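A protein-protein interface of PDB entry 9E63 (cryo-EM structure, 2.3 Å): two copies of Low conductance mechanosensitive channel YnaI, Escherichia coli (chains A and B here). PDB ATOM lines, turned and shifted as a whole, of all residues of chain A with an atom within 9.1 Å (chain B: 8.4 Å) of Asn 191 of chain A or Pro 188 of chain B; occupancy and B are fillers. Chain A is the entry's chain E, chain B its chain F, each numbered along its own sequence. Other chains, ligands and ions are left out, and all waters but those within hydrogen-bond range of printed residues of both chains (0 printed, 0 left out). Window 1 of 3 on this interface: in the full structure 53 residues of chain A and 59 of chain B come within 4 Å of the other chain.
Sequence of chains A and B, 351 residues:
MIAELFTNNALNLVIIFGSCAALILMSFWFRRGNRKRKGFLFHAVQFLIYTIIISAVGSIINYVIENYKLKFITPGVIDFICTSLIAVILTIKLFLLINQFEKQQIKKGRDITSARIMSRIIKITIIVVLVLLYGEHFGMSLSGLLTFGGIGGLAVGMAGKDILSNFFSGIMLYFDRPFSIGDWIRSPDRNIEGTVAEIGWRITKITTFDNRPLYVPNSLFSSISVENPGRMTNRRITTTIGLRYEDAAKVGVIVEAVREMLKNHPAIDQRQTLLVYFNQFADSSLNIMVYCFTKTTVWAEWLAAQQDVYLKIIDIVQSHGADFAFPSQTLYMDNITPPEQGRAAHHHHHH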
ATOM      1  N   ILE A 185      -3.884 -15.377 -14.721  1.00  0.00           N
ATOM      2  CA  ILE A 185      -3.138 -14.961 -13.544  1.00  0.00           C
ATOM      3  C   ILE A 185      -2.692 -13.514 -13.715  1.00  0.00           C
ATOM      4  O   ILE A 185      -2.746 -12.943 -14.802  1.00  0.00           O
ATOM      5  CB  ILE A 185      -1.927 -15.871 -13.249  1.00  0.00           C
ATOM      6  CG1 ILE A 185      -0.907 -15.808 -14.386  1.00  0.00           C
ATOM      7  CG2 ILE A 185      -2.375 -17.296 -12.973  1.00  0.00           C
ATOM      8  CD1 ILE A 185       0.433 -16.386 -14.023  1.00  0.00           C
ATOM      9  N   ARG A 186      -2.231 -12.934 -12.613  1.00  0.00           N
ATOM     10  CA  ARG A 186      -1.966 -11.506 -12.527  1.00  0.00           C
ATOM     11  C   ARG A 186      -0.990 -11.272 -11.384  1.00  0.00           C
ATOM     12  O   ARG A 186      -0.701 -12.174 -10.598  1.00  0.00           O
ATOM     13  CB  ARG A 186      -3.265 -10.725 -12.309  1.00  0.00           C
ATOM     14  CG  ARG A 186      -3.331  -9.396 -13.000  1.00  0.00           C
ATOM     15  CD  ARG A 186      -4.557  -8.628 -12.546  1.00  0.00           C
ATOM     16  NE  ARG A 186      -4.483  -8.294 -11.130  1.00  0.00           N
ATOM     17  CZ  ARG A 186      -3.785  -7.284 -10.633  1.00  0.00           C
ATOM     18  NH1 ARG A 186      -3.096  -6.469 -11.414  1.00  0.00           N
ATOM     19  NH2 ARG A 186      -3.775  -7.088  -9.320  1.00  0.00           N
ATOM     20  N   SER A 187      -0.481 -10.044 -11.300  1.00  0.00           N
ATOM     21  CA  SER A 187       0.394  -9.685 -10.204  1.00  0.00           C
ATOM     22  C   SER A 187       0.353  -8.182  -9.971  1.00  0.00           C
ATOM     23  O   SER A 187       0.401  -7.416 -10.944  1.00  0.00           O
ATOM     24  CB  SER A 187       1.834 -10.124 -10.460  1.00  0.00           C
ATOM     25  OG  SER A 187       2.678  -9.727  -9.399  1.00  0.00           O
ATOM     26  N   PRO A 188       0.257  -7.731  -8.719  1.00  0.00           N
ATOM     27  CA  PRO A 188       0.383  -6.293  -8.442  1.00  0.00           C
ATOM     28  C   PRO A 188       1.810  -5.777  -8.486  1.00  0.00           C
ATOM     29  O   PRO A 188       2.005  -4.555  -8.477  1.00  0.00           O
ATOM     30  CB  PRO A 188      -0.205  -6.161  -7.031  1.00  0.00           C
ATOM     31  CG  PRO A 188       0.003  -7.494  -6.415  1.00  0.00           C
ATOM     32  CD  PRO A 188      -0.124  -8.498  -7.521  1.00  0.00           C
ATOM     33  N   ASP A 189       2.809  -6.656  -8.543  1.00  0.00           N
ATOM     34  CA  ASP A 189       4.214  -6.263  -8.522  1.00  0.00           C
ATOM     35  C   ASP A 189       4.834  -6.154  -9.909  1.00  0.00           C
ATOM     36  O   ASP A 189       5.641  -5.250 -10.145  1.00  0.00           O
ATOM     37  CB  ASP A 189       5.024  -7.255  -7.683  1.00  0.00           C
ATOM     38  CG  ASP A 189       4.521  -7.360  -6.260  1.00  0.00           C
ATOM     39  OD1 ASP A 189       4.309  -6.310  -5.623  1.00  0.00           O
ATOM     40  OD2 ASP A 189       4.333  -8.494  -5.774  1.00  0.00           O
ATOM     41  N   ARG A 190       4.498  -7.059 -10.826  1.00  0.00           N
ATOM     42  CA  ARG A 190       5.019  -7.038 -12.185  1.00  0.00           C
ATOM     43  C   ARG A 190       3.886  -7.286 -13.168  1.00  0.00           C
ATOM     44  O   ARG A 190       2.808  -7.757 -12.800  1.00  0.00           O
ATOM     45  CB  ARG A 190       6.118  -8.090 -12.406  1.00  0.00           C
ATOM     46  CG  ARG A 190       7.108  -8.233 -11.274  1.00  0.00           C
ATOM     47  CD  ARG A 190       8.358  -7.416 -11.528  1.00  0.00           C
ATOM     48  NE  ARG A 190       9.012  -7.776 -12.778  1.00  0.00           N
ATOM     49  CZ  ARG A 190      10.218  -8.319 -12.862  1.00  0.00           C
ATOM     50  NH1 ARG A 190      10.926  -8.597 -11.782  1.00  0.00           N
ATOM     51  NH2 ARG A 190      10.726  -8.587 -14.061  1.00  0.00           N
ATOM     52  N   ASN A 191       4.147  -6.966 -14.433  1.00  0.00           N
ATOM     53  CA  ASN A 191       3.192  -7.199 -15.514  1.00  0.00           C
ATOM     54  C   ASN A 191       3.424  -8.599 -16.064  1.00  0.00           C
ATOM     55  O   ASN A 191       4.365  -8.834 -16.823  1.00  0.00           O
ATOM     56  CB  ASN A 191       3.342  -6.136 -16.597  1.00  0.00           C
ATOM     57  CG  ASN A 191       2.209  -6.159 -17.600  1.00  0.00           C
ATOM     58  OD1 ASN A 191       1.348  -7.035 -17.564  1.00  0.00           O
ATOM     59  ND2 ASN A 191       2.203  -5.191 -18.504  1.00  0.00           N
ATOM     60  N   ILE A 192       2.565  -9.538 -15.671  1.00  0.00           N
ATOM     61  CA  ILE A 192       2.641 -10.921 -16.132  1.00  0.00           C
ATOM     62  C   ILE A 192       1.260 -11.385 -16.573  1.00  0.00           C
ATOM     63  O   ILE A 192       1.013 -12.588 -16.694  1.00  0.00           O
ATOM     64  CB  ILE A 192       3.198 -11.848 -15.035  1.00  0.00           C
ATOM     65  CG1 ILE A 192       2.307 -11.791 -13.794  1.00  0.00           C
ATOM     66  CG2 ILE A 192       4.628 -11.481 -14.690  1.00  0.00           C
ATOM     67  CD1 ILE A 192       2.362 -13.032 -12.944  1.00  0.00           C
ATOM     68  N   GLU A 193       0.352 -10.439 -16.802  1.00  0.00           N
ATOM     69  CA  GLU A 193      -1.060 -10.772 -16.949  1.00  0.00           C
ATOM     70  C   GLU A 193      -1.330 -11.572 -18.220  1.00  0.00           C
ATOM     71  O   GLU A 193      -0.805 -11.267 -19.294  1.00  0.00           O
ATOM     72  CB  GLU A 193      -1.900  -9.498 -16.945  1.00  0.00           C
ATOM     73  CG  GLU A 193      -3.387  -9.744 -17.097  1.00  0.00           C
ATOM     74  CD  GLU A 193      -4.226  -8.783 -16.289  1.00  0.00           C
ATOM     75  OE1 GLU A 193      -3.713  -7.710 -15.916  1.00  0.00           O
ATOM     76  OE2 GLU A 193      -5.402  -9.099 -16.024  1.00  0.00           O
ATOM     77  N   GLY A 194      -2.167 -12.589 -18.089  1.00  0.00           N
ATOM     78  CA  GLY A 194      -2.554 -13.429 -19.202  1.00  0.00           C
ATOM     79  C   GLY A 194      -2.979 -14.790 -18.690  1.00  0.00           C
ATOM     80  O   GLY A 194      -3.107 -15.010 -17.492  1.00  0.00           O
ATOM     81  N   ILE A 206       2.968 -17.508 -21.219  1.00  0.00           N
ATOM     82  CA  ILE A 206       1.660 -16.952 -20.903  1.00  0.00           C
ATOM     83  C   ILE A 206       1.115 -16.274 -22.152  1.00  0.00           C
ATOM     84  O   ILE A 206       1.840 -15.539 -22.828  1.00  0.00           O
ATOM     85  CB  ILE A 206       1.756 -15.945 -19.737  1.00  0.00           C
ATOM     86  CG1 ILE A 206       1.891 -16.679 -18.405  1.00  0.00           C
ATOM     87  CG2 ILE A 206       0.572 -15.004 -19.725  1.00  0.00           C
ATOM     88  CD1 ILE A 206       2.726 -15.948 -17.402  1.00  0.00           C
ATOM     89  N   THR A 208      -1.021 -13.426 -23.574  1.00  0.00           N
ATOM     90  CA  THR A 208      -1.584 -12.155 -23.143  1.00  0.00           C
ATOM     91  C   THR A 208      -2.961 -11.953 -23.771  1.00  0.00           C
ATOM     92  O   THR A 208      -3.415 -12.724 -24.617  1.00  0.00           O
ATOM     93  CB  THR A 208      -0.653 -10.999 -23.502  1.00  0.00           C
ATOM     94  OG1 THR A 208      -0.742 -10.726 -24.902  1.00  0.00           O
ATOM     95  CG2 THR A 208       0.780 -11.336 -23.151  1.00  0.00           C
ATOM     96  N   PHE A 209      -3.640 -10.891 -23.348  1.00  0.00           N
ATOM     97  CA  PHE A 209      -5.004 -10.659 -23.800  1.00  0.00           C
ATOM     98  C   PHE A 209      -5.085  -9.987 -25.163  1.00  0.00           C
ATOM     99  O   PHE A 209      -6.190  -9.840 -25.691  1.00  0.00           O
ATOM    100  CB  PHE A 209      -5.765  -9.847 -22.752  1.00  0.00           C
ATOM    101  CG  PHE A 209      -6.256 -10.675 -21.604  1.00  0.00           C
ATOM    102  CD1 PHE A 209      -7.262 -11.606 -21.789  1.00  0.00           C
ATOM    103  CD2 PHE A 209      -5.693 -10.547 -20.348  1.00  0.00           C
ATOM    104  CE1 PHE A 209      -7.707 -12.381 -20.741  1.00  0.00           C
ATOM    105  CE2 PHE A 209      -6.136 -11.322 -19.295  1.00  0.00           C
ATOM    106  CZ  PHE A 209      -7.142 -12.239 -19.491  1.00  0.00           C
ATOM    107  N   ASP A 210      -3.960  -9.586 -25.753  1.00  0.00           N
ATOM    108  CA  ASP A 210      -3.922  -9.225 -27.163  1.00  0.00           C
ATOM    109  C   ASP A 210      -3.349 -10.345 -28.022  1.00  0.00           C
ATOM    110  O   ASP A 210      -2.867 -10.085 -29.128  1.00  0.00           O
ATOM    111  CB  ASP A 210      -3.134  -7.933 -27.378  1.00  0.00           C
ATOM    112  CG  ASP A 210      -1.914  -7.836 -26.501  1.00  0.00           C
ATOM    113  OD1 ASP A 210      -1.460  -8.880 -25.993  1.00  0.00           O
ATOM    114  OD2 ASP A 210      -1.402  -6.714 -26.327  1.00  0.00           O
ATOM    115  N   PRO A 213       2.476 -14.110 -27.109  1.00  0.00           N
ATOM    116  CA  PRO A 213       3.179 -14.914 -26.103  1.00  0.00           C
ATOM    117  C   PRO A 213       4.137 -14.075 -25.271  1.00  0.00           C
ATOM    118  O   PRO A 213       4.824 -13.187 -25.778  1.00  0.00           O
ATOM    119  CB  PRO A 213       3.931 -15.948 -26.946  1.00  0.00           C
ATOM    120  CG  PRO A 213       4.136 -15.285 -28.250  1.00  0.00           C
ATOM    121  CD  PRO A 213       2.977 -14.360 -28.470  1.00  0.00           C
ATOM    122  N   LEU A 214       4.181 -14.379 -23.978  1.00  0.00           N
ATOM    123  CA  LEU A 214       5.028 -13.691 -23.018  1.00  0.00           C
ATOM    124  C   LEU A 214       5.778 -14.738 -22.209  1.00  0.00           C
ATOM    125  O   LEU A 214       5.174 -15.692 -21.715  1.00  0.00           O
ATOM    126  CB  LEU A 214       4.193 -12.789 -22.104  1.00  0.00           C
ATOM    127  CG  LEU A 214       4.881 -12.035 -20.969  1.00  0.00           C
ATOM    128  CD1 LEU A 214       5.587 -10.800 -21.488  1.00  0.00           C
ATOM    129  CD2 LEU A 214       3.864 -11.660 -19.909  1.00  0.00           C
ATOM    130  N   TYR A 215       7.088 -14.565 -22.086  1.00  0.00           N
ATOM    131  CA  TYR A 215       7.956 -15.544 -21.440  1.00  0.00           C
ATOM    132  C   TYR A 215       8.448 -14.959 -20.125  1.00  0.00           C
ATOM    133  O   TYR A 215       9.206 -13.986 -20.117  1.00  0.00           O
ATOM    134  CB  TYR A 215       9.115 -15.919 -22.358  1.00  0.00           C
ATOM    135  CG  TYR A 215       8.660 -16.410 -23.711  1.00  0.00           C
ATOM    136  CD1 TYR A 215       8.364 -17.745 -23.919  1.00  0.00           C
ATOM    137  CD2 TYR A 215       8.514 -15.536 -24.775  1.00  0.00           C
ATOM    138  CE1 TYR A 215       7.943 -18.198 -25.147  1.00  0.00           C
ATOM    139  CE2 TYR A 215       8.095 -15.977 -26.007  1.00  0.00           C
ATOM    140  CZ  TYR A 215       7.809 -17.311 -26.188  1.00  0.00           C
ATOM    141  OH  TYR A 215       7.391 -17.762 -27.415  1.00  0.00           O
ATOM    142  N   VAL A 216       8.029 -15.557 -19.019  1.00  0.00           N
ATOM    143  CA  VAL A 216       8.300 -15.053 -17.678  1.00  0.00           C
ATOM    144  C   VAL A 216       9.350 -15.951 -17.038  1.00  0.00           C
ATOM    145  O   VAL A 216       9.138 -17.166 -16.943  1.00  0.00           O
ATOM    146  CB  VAL A 216       7.022 -15.005 -16.825  1.00  0.00           C
ATOM    147  CG1 VAL A 216       7.329 -14.476 -15.440  1.00  0.00           C
ATOM    148  CG2 VAL A 216       5.971 -14.153 -17.502  1.00  0.00           C
ATOM    149  N   PRO A 217      10.491 -15.417 -16.605  1.00  0.00           N
ATOM    150  CA  PRO A 217      11.456 -16.243 -15.871  1.00  0.00           C
ATOM    151  C   PRO A 217      10.833 -16.801 -14.599  1.00  0.00           C
ATOM    152  O   PRO A 217      10.071 -16.122 -13.911  1.00  0.00           O
ATOM    153  CB  PRO A 217      12.597 -15.266 -15.560  1.00  0.00           C
ATOM    154  CG  PRO A 217      12.416 -14.144 -16.514  1.00  0.00           C
ATOM    155  CD  PRO A 217      10.949 -14.027 -16.744  1.00  0.00           C
ATOM    156  N   LEU A 220      10.797 -15.232 -10.798  1.00  0.00           N
ATOM    157  CA  LEU A 220       9.821 -14.232 -10.380  1.00  0.00           C
ATOM    158  C   LEU A 220       8.775 -14.823  -9.448  1.00  0.00           C
ATOM    159  O   LEU A 220       8.300 -14.137  -8.538  1.00  0.00           O
ATOM    160  CB  LEU A 220       9.126 -13.615 -11.593  1.00  0.00           C
ATOM    161  CG  LEU A 220       9.933 -12.786 -12.590  1.00  0.00           C
ATOM    162  CD1 LEU A 220       9.014 -11.823 -13.312  1.00  0.00           C
ATOM    163  CD2 LEU A 220      11.055 -12.046 -11.899  1.00  0.00           C
ATOM    164  N   PHE A 221       8.411 -16.087  -9.648  1.00  0.00           N
ATOM    165  CA  PHE A 221       7.364 -16.686  -8.838  1.00  0.00           C
ATOM    166  C   PHE A 221       7.828 -17.023  -7.428  1.00  0.00           C
ATOM    167  O   PHE A 221       7.036 -17.555  -6.647  1.00  0.00           O
ATOM    168  CB  PHE A 221       6.819 -17.925  -9.543  1.00  0.00           C
ATOM    169  CG  PHE A 221       6.197 -17.625 -10.876  1.00  0.00           C
ATOM    170  CD1 PHE A 221       5.032 -16.886 -10.957  1.00  0.00           C
ATOM    171  CD2 PHE A 221       6.793 -18.052 -12.047  1.00  0.00           C
ATOM    172  CE1 PHE A 221       4.464 -16.595 -12.178  1.00  0.00           C
ATOM    173  CE2 PHE A 221       6.231 -17.762 -13.269  1.00  0.00           C
ATOM    174  CZ  PHE A 221       5.064 -17.034 -13.335  1.00  0.00           C
ATOM    175  N   ILE A 224       7.245 -12.507  -5.940  1.00  0.00           N
ATOM    176  CA  ILE A 224       6.125 -11.607  -6.166  1.00  0.00           C
ATOM    177  C   ILE A 224       4.837 -12.303  -5.754  1.00  0.00           C
ATOM    178  O   ILE A 224       4.738 -13.529  -5.741  1.00  0.00           O
ATOM    179  CB  ILE A 224       6.037 -11.133  -7.633  1.00  0.00           C
ATOM    180  CG1 ILE A 224       5.654 -12.295  -8.546  1.00  0.00           C
ATOM    181  CG2 ILE A 224       7.347 -10.512  -8.074  1.00  0.00           C
ATOM    182  CD1 ILE A 224       5.522 -11.912  -9.989  1.00  0.00           C
ATOM    183  N   SER A 225       3.843 -11.493  -5.405  1.00  0.00           N
ATOM    184  CA  SER A 225       2.513 -12.008  -5.111  1.00  0.00           C
ATOM    185  C   SER A 225       1.783 -12.302  -6.412  1.00  0.00           C
ATOM    186  O   SER A 225       1.807 -11.492  -7.342  1.00  0.00           O
ATOM    187  CB  SER A 225       1.722 -11.004  -4.275  1.00  0.00           C
ATOM    188  OG  SER A 225       2.349 -10.773  -3.029  1.00  0.00           O
ATOM    189  N   ILE B 185      10.320  -8.075 -30.729  1.00  0.00           N
ATOM    190  CA  ILE B 185      10.221  -8.406 -29.313  1.00  0.00           C
ATOM    191  C   ILE B 185      10.055  -7.123 -28.507  1.00  0.00           C
ATOM    192  O   ILE B 185      10.245  -6.015 -29.002  1.00  0.00           O
ATOM    193  CB  ILE B 185      11.426  -9.220 -28.802  1.00  0.00           C
ATOM    194  CG1 ILE B 185      12.717  -8.412 -28.912  1.00  0.00           C
ATOM    195  CG2 ILE B 185      11.536 -10.541 -29.538  1.00  0.00           C
ATOM    196  CD1 ILE B 185      13.854  -8.994 -28.118  1.00  0.00           C
ATOM    197  N   ARG B 186       9.710  -7.303 -27.238  1.00  0.00           N
ATOM    198  CA  ARG B 186       9.290  -6.213 -26.371  1.00  0.00           C
ATOM    199  C   ARG B 186       9.468  -6.660 -24.929  1.00  0.00           C
ATOM    200  O   ARG B 186       9.724  -7.835 -24.653  1.00  0.00           O
ATOM    201  CB  ARG B 186       7.836  -5.826 -26.651  1.00  0.00           C
ATOM    202  CG  ARG B 186       7.538  -4.362 -26.557  1.00  0.00           C
ATOM    203  CD  ARG B 186       6.044  -4.118 -26.617  1.00  0.00           C
ATOM    204  NE  ARG B 186       5.357  -4.705 -25.475  1.00  0.00           N
ATOM    205  CZ  ARG B 186       5.301  -4.152 -24.271  1.00  0.00           C
ATOM    206  NH1 ARG B 186       5.867  -2.984 -24.019  1.00  0.00           N
ATOM    207  NH2 ARG B 186       4.665  -4.790 -23.295  1.00  0.00           N
ATOM    208  N   SER B 187       9.330  -5.711 -24.007  1.00  0.00           N
ATOM    209  CA  SER B 187       9.402  -6.041 -22.599  1.00  0.00           C
ATOM    210  C   SER B 187       8.653  -5.003 -21.777  1.00  0.00           C
ATOM    211  O   SER B 187       8.812  -3.800 -22.028  1.00  0.00           O
ATOM    212  CB  SER B 187      10.846  -6.132 -22.113  1.00  0.00           C
ATOM    213  OG  SER B 187      10.895  -6.418 -20.730  1.00  0.00           O
ATOM    214  N   PRO B 188       7.832  -5.423 -20.811  1.00  0.00           N
ATOM    215  CA  PRO B 188       7.224  -4.455 -19.888  1.00  0.00           C
ATOM    216  C   PRO B 188       8.173  -3.939 -18.819  1.00  0.00           C
ATOM    217  O   PRO B 188       7.810  -2.999 -18.102  1.00  0.00           O
ATOM    218  CB  PRO B 188       6.073  -5.250 -19.262  1.00  0.00           C
ATOM    219  CG  PRO B 188       6.511  -6.663 -19.348  1.00  0.00           C
ATOM    220  CD  PRO B 188       7.316  -6.786 -20.607  1.00  0.00           C
ATOM    221  N   ASP B 189       9.370  -4.508 -18.694  1.00  0.00           N
ATOM    222  CA  ASP B 189      10.323  -4.131 -17.657  1.00  0.00           C
ATOM    223  C   ASP B 189      11.387  -3.153 -18.138  1.00  0.00           C
ATOM    224  O   ASP B 189      11.741  -2.227 -17.405  1.00  0.00           O
ATOM    225  CB  ASP B 189      11.006  -5.380 -17.092  1.00  0.00           C
ATOM    226  CG  ASP B 189      10.021  -6.376 -16.524  1.00  0.00           C
ATOM    227  OD1 ASP B 189       9.122  -5.960 -15.769  1.00  0.00           O
ATOM    228  OD2 ASP B 189      10.142  -7.577 -16.831  1.00  0.00           O
ATOM    229  N   ARG B 190      11.919  -3.344 -19.343  1.00  0.00           N
ATOM    230  CA  ARG B 190      12.927  -2.466 -19.916  1.00  0.00           C
ATOM    231  C   ARG B 190      12.553  -2.137 -21.352  1.00  0.00           C
ATOM    232  O   ARG B 190      11.714  -2.797 -21.966  1.00  0.00           O
ATOM    233  CB  ARG B 190      14.329  -3.094 -19.888  1.00  0.00           C
ATOM    234  CG  ARG B 190      14.687  -3.813 -18.609  1.00  0.00           C
ATOM    235  CD  ARG B 190      15.491  -2.921 -17.683  1.00  0.00           C
ATOM    236  NE  ARG B 190      16.712  -2.429 -18.306  1.00  0.00           N
ATOM    237  CZ  ARG B 190      17.935  -2.710 -17.878  1.00  0.00           C
ATOM    238  NH1 ARG B 190      18.138  -3.495 -16.837  1.00  0.00           N
ATOM    239  NH2 ARG B 190      18.981  -2.187 -18.513  1.00  0.00           N
ATOM    240  N   ASN B 191      13.193  -1.101 -21.888  1.00  0.00           N
ATOM    241  CA  ASN B 191      12.994  -0.690 -23.276  1.00  0.00           C
ATOM    242  C   ASN B 191      13.979  -1.457 -24.151  1.00  0.00           C
ATOM    243  O   ASN B 191      15.167  -1.136 -24.197  1.00  0.00           O
ATOM    244  CB  ASN B 191      13.166   0.816 -23.420  1.00  0.00           C
ATOM    245  CG  ASN B 191      12.670   1.337 -24.751  1.00  0.00           C
ATOM    246  OD1 ASN B 191      12.322   0.566 -25.642  1.00  0.00           O
ATOM    247  ND2 ASN B 191      12.635   2.653 -24.892  1.00  0.00           N
ATOM    248  N   ILE B 192      13.485  -2.485 -24.839  1.00  0.00           N
ATOM    249  CA  ILE B 192      14.296  -3.297 -25.740  1.00  0.00           C
ATOM    250  C   ILE B 192      13.567  -3.486 -27.063  1.00  0.00           C
ATOM    251  O   ILE B 192      13.910  -4.380 -27.842  1.00  0.00           O
ATOM    252  CB  ILE B 192      14.634  -4.662 -25.112  1.00  0.00           C
ATOM    253  CG1 ILE B 192      13.352  -5.414 -24.746  1.00  0.00           C
ATOM    254  CG2 ILE B 192      15.524  -4.495 -23.897  1.00  0.00           C
ATOM    255  CD1 ILE B 192      13.517  -6.905 -24.660  1.00  0.00           C
ATOM    256  N   ILE B 224      14.111 -10.529 -16.998  1.00  0.00           N
ATOM    257  CA  ILE B 224      12.949  -9.749 -17.398  1.00  0.00           C
ATOM    258  C   ILE B 224      12.020 -10.626 -18.226  1.00  0.00           C
ATOM    259  O   ILE B 224      12.434 -11.609 -18.844  1.00  0.00           O
ATOM    260  CB  ILE B 224      13.329  -8.480 -18.189  1.00  0.00           C
ATOM    261  CG1 ILE B 224      13.886  -8.856 -19.561  1.00  0.00           C
ATOM    262  CG2 ILE B 224      14.320  -7.637 -17.411  1.00  0.00           C
ATOM    263  CD1 ILE B 224      14.240  -7.681 -20.421  1.00  0.00           C
ATOM    264  N   SER B 225      10.745 -10.256 -18.227  1.00  0.00           N
ATOM    265  CA  SER B 225       9.767 -10.905 -19.086  1.00  0.00           C
ATOM    266  C   SER B 225       9.906 -10.375 -20.505  1.00  0.00           C
ATOM    267  O   SER B 225      10.001  -9.166 -20.716  1.00  0.00           O
ATOM    268  CB  SER B 225       8.349 -10.666 -18.570  1.00  0.00           C
ATOM    269  OG  SER B 225       8.169 -11.240 -17.292  1.00  0.00           O
ATOM    270  N   VAL B 226       9.919 -11.282 -21.474  1.00  0.00           N
ATOM    271  CA  VAL B 226      10.084 -10.930 -22.878  1.00  0.00           C
ATOM    272  C   VAL B 226       8.796 -11.278 -23.607  1.00  0.00           C
ATOM    273  O   VAL B 226       8.327 -12.419 -23.549  1.00  0.00           O
ATOM    274  CB  VAL B 226      11.290 -11.646 -23.505  1.00  0.00           C
ATOM    275  CG1 VAL B 226      11.370 -11.344 -24.988  1.00  0.00           C
ATOM    276  CG2 VAL B 226      12.567 -11.230 -22.809  1.00  0.00           C
ATOM    277  N   GLU B 227       8.226 -10.293 -24.285  1.00  0.00           N
ATOM    278  CA  GLU B 227       7.049 -10.476 -25.115  1.00  0.00           C
ATOM    279  C   GLU B 227       7.471 -10.564 -26.573  1.00  0.00           C
ATOM    280  O   GLU B 227       8.443  -9.935 -26.993  1.00  0.00           O
ATOM    281  CB  GLU B 227       6.064  -9.325 -24.909  1.00  0.00           C
ATOM    282  CG  GLU B 227       4.727  -9.497 -25.589  1.00  0.00           C
ATOM    283  CD  GLU B 227       3.792  -8.340 -25.318  1.00  0.00           C
ATOM    284  OE1 GLU B 227       3.483  -7.591 -26.264  1.00  0.00           O
ATOM    285  OE2 GLU B 227       3.360  -8.183 -24.158  1.00  0.00           O
ATOM    286  N   ASN B 228       6.734 -11.352 -27.347  1.00  0.00           N
ATOM    287  CA  ASN B 228       7.058 -11.612 -28.748  1.00  0.00           C
ATOM    288  C   ASN B 228       5.852 -11.267 -29.611  1.00  0.00           C
ATOM    289  O   ASN B 228       5.095 -12.152 -30.023  1.00  0.00           O
ATOM    290  CB  ASN B 228       7.485 -13.066 -28.946  1.00  0.00           C
ATOM    291  CG  ASN B 228       8.379 -13.257 -30.152  1.00  0.00           C
ATOM    292  OD1 ASN B 228       8.250 -12.563 -31.153  1.00  0.00           O
ATOM    293  ND2 ASN B 228       9.296 -14.205 -30.059  1.00  0.00           N
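Arg 190 of chain A touches Asp 189 of chain B, but with the chains exchanged Asp 189 of chain A does not touch Arg 190 of chain B (11.3 Å). Asn 191 of chain A touches Pro 188 of chain B, but with the chains exchanged Pro 188 of chain A does not touch Asn 191 of chain B (17.8 Å). Positions printed for both chains: 185, 186, 187, 188, 189, 190, 191, 192, 224 and 225.
Asn 191 of chain A touches one residue of chain B. Of the printed residues of chain B, Leu 214 of chain A touches Val 226 (3.6 Å) and Glu 227 (3.8 Å). Printed residues of chain B within 4 Å of Tyr 215 of chain A: Ser 225 and Val 226. Ser 187 of chain B touches none of the printed residues of chain A. Of chain A, only Asn 191 comes within 4 Å of Pro 188 of chain B. Of chain A, only Arg 190 (3.0 Å) comes within 4 Å of Asp 189 of chain B. Of the printed residues of chain A, Ser 225 of chain B touches Tyr 215, Val 216 and Pro 217.
The side-chain carboxylate of Asp 189 of chain B is in salt-bridge range of the guanidinium group of Arg 190 of chain A (3.0 Å). O of Pro 213 of chain A is in hydrogen-bond range of N of Asn 228 of chain B, 3.1 Å away. The backbone NH of Tyr 215 of chain A lies within hydrogen-bond range of the backbone carbonyl oxygen of Val 226 of chain B (2.9 Å).
Among the printed residues, pairs that only touch across the chains: Tyr 215 of chain A with Ser 225 of chain B, Pro 217 of chain A with Ile 224 of chain B, Pro 213 of chain A with Glu 227 of chain B, Leu 214 of chain A with Val 226 of chain B, Val 216 of chain A with Ser 225 of chain B, Leu 214 of chain A with Glu 227 of chain B, Asn 191 of chain A with Pro 188 of chain B and Pro 217 of chain A with Ser 225 of chain B.
Of the 23 printed residues of chain A, 7 touch a printed residue of chain B. Printed residues of chain A that touch a printed residue of chain B: Arg 190, Asn 191, Pro 213, Leu 214, Tyr 215, Val 216 and Pro 217. Among the printed residues, 11 pairs touch across the chains. Among the printed residues, Asp or Glu carboxylates within 4 Å of a Lys or Arg side-chain nitrogen of the other chain: Arg 190 of chain A with Asp 189 of chain B.
O of Ile 206 of chain A lies within hydrogen-bond range of N of Leu 214 of chain A, at 2.9 Å. The guanidinium group (NE) of Arg 186 of chain B is in salt-bridge range of the side-chain carboxylate (OE1) of Glu 227 of chain B (3.5 Å). The backbone NH (N) of Asp 189 of chain B is in hydrogen-bond range of the side-chain hydroxyl (OG) of Ser 187 of chain B, 3.2 Å away. The side-chain hydroxyl (OG) of Ser 187 of chain B lies within hydrogen-bond range of the backbone carbonyl oxygen (O) of Ser 225 of chain B, 2.9 Å away. N of Ser 225 of chain B sits at hydrogen-bond distance from OD2 of Asp 189 of chain B.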
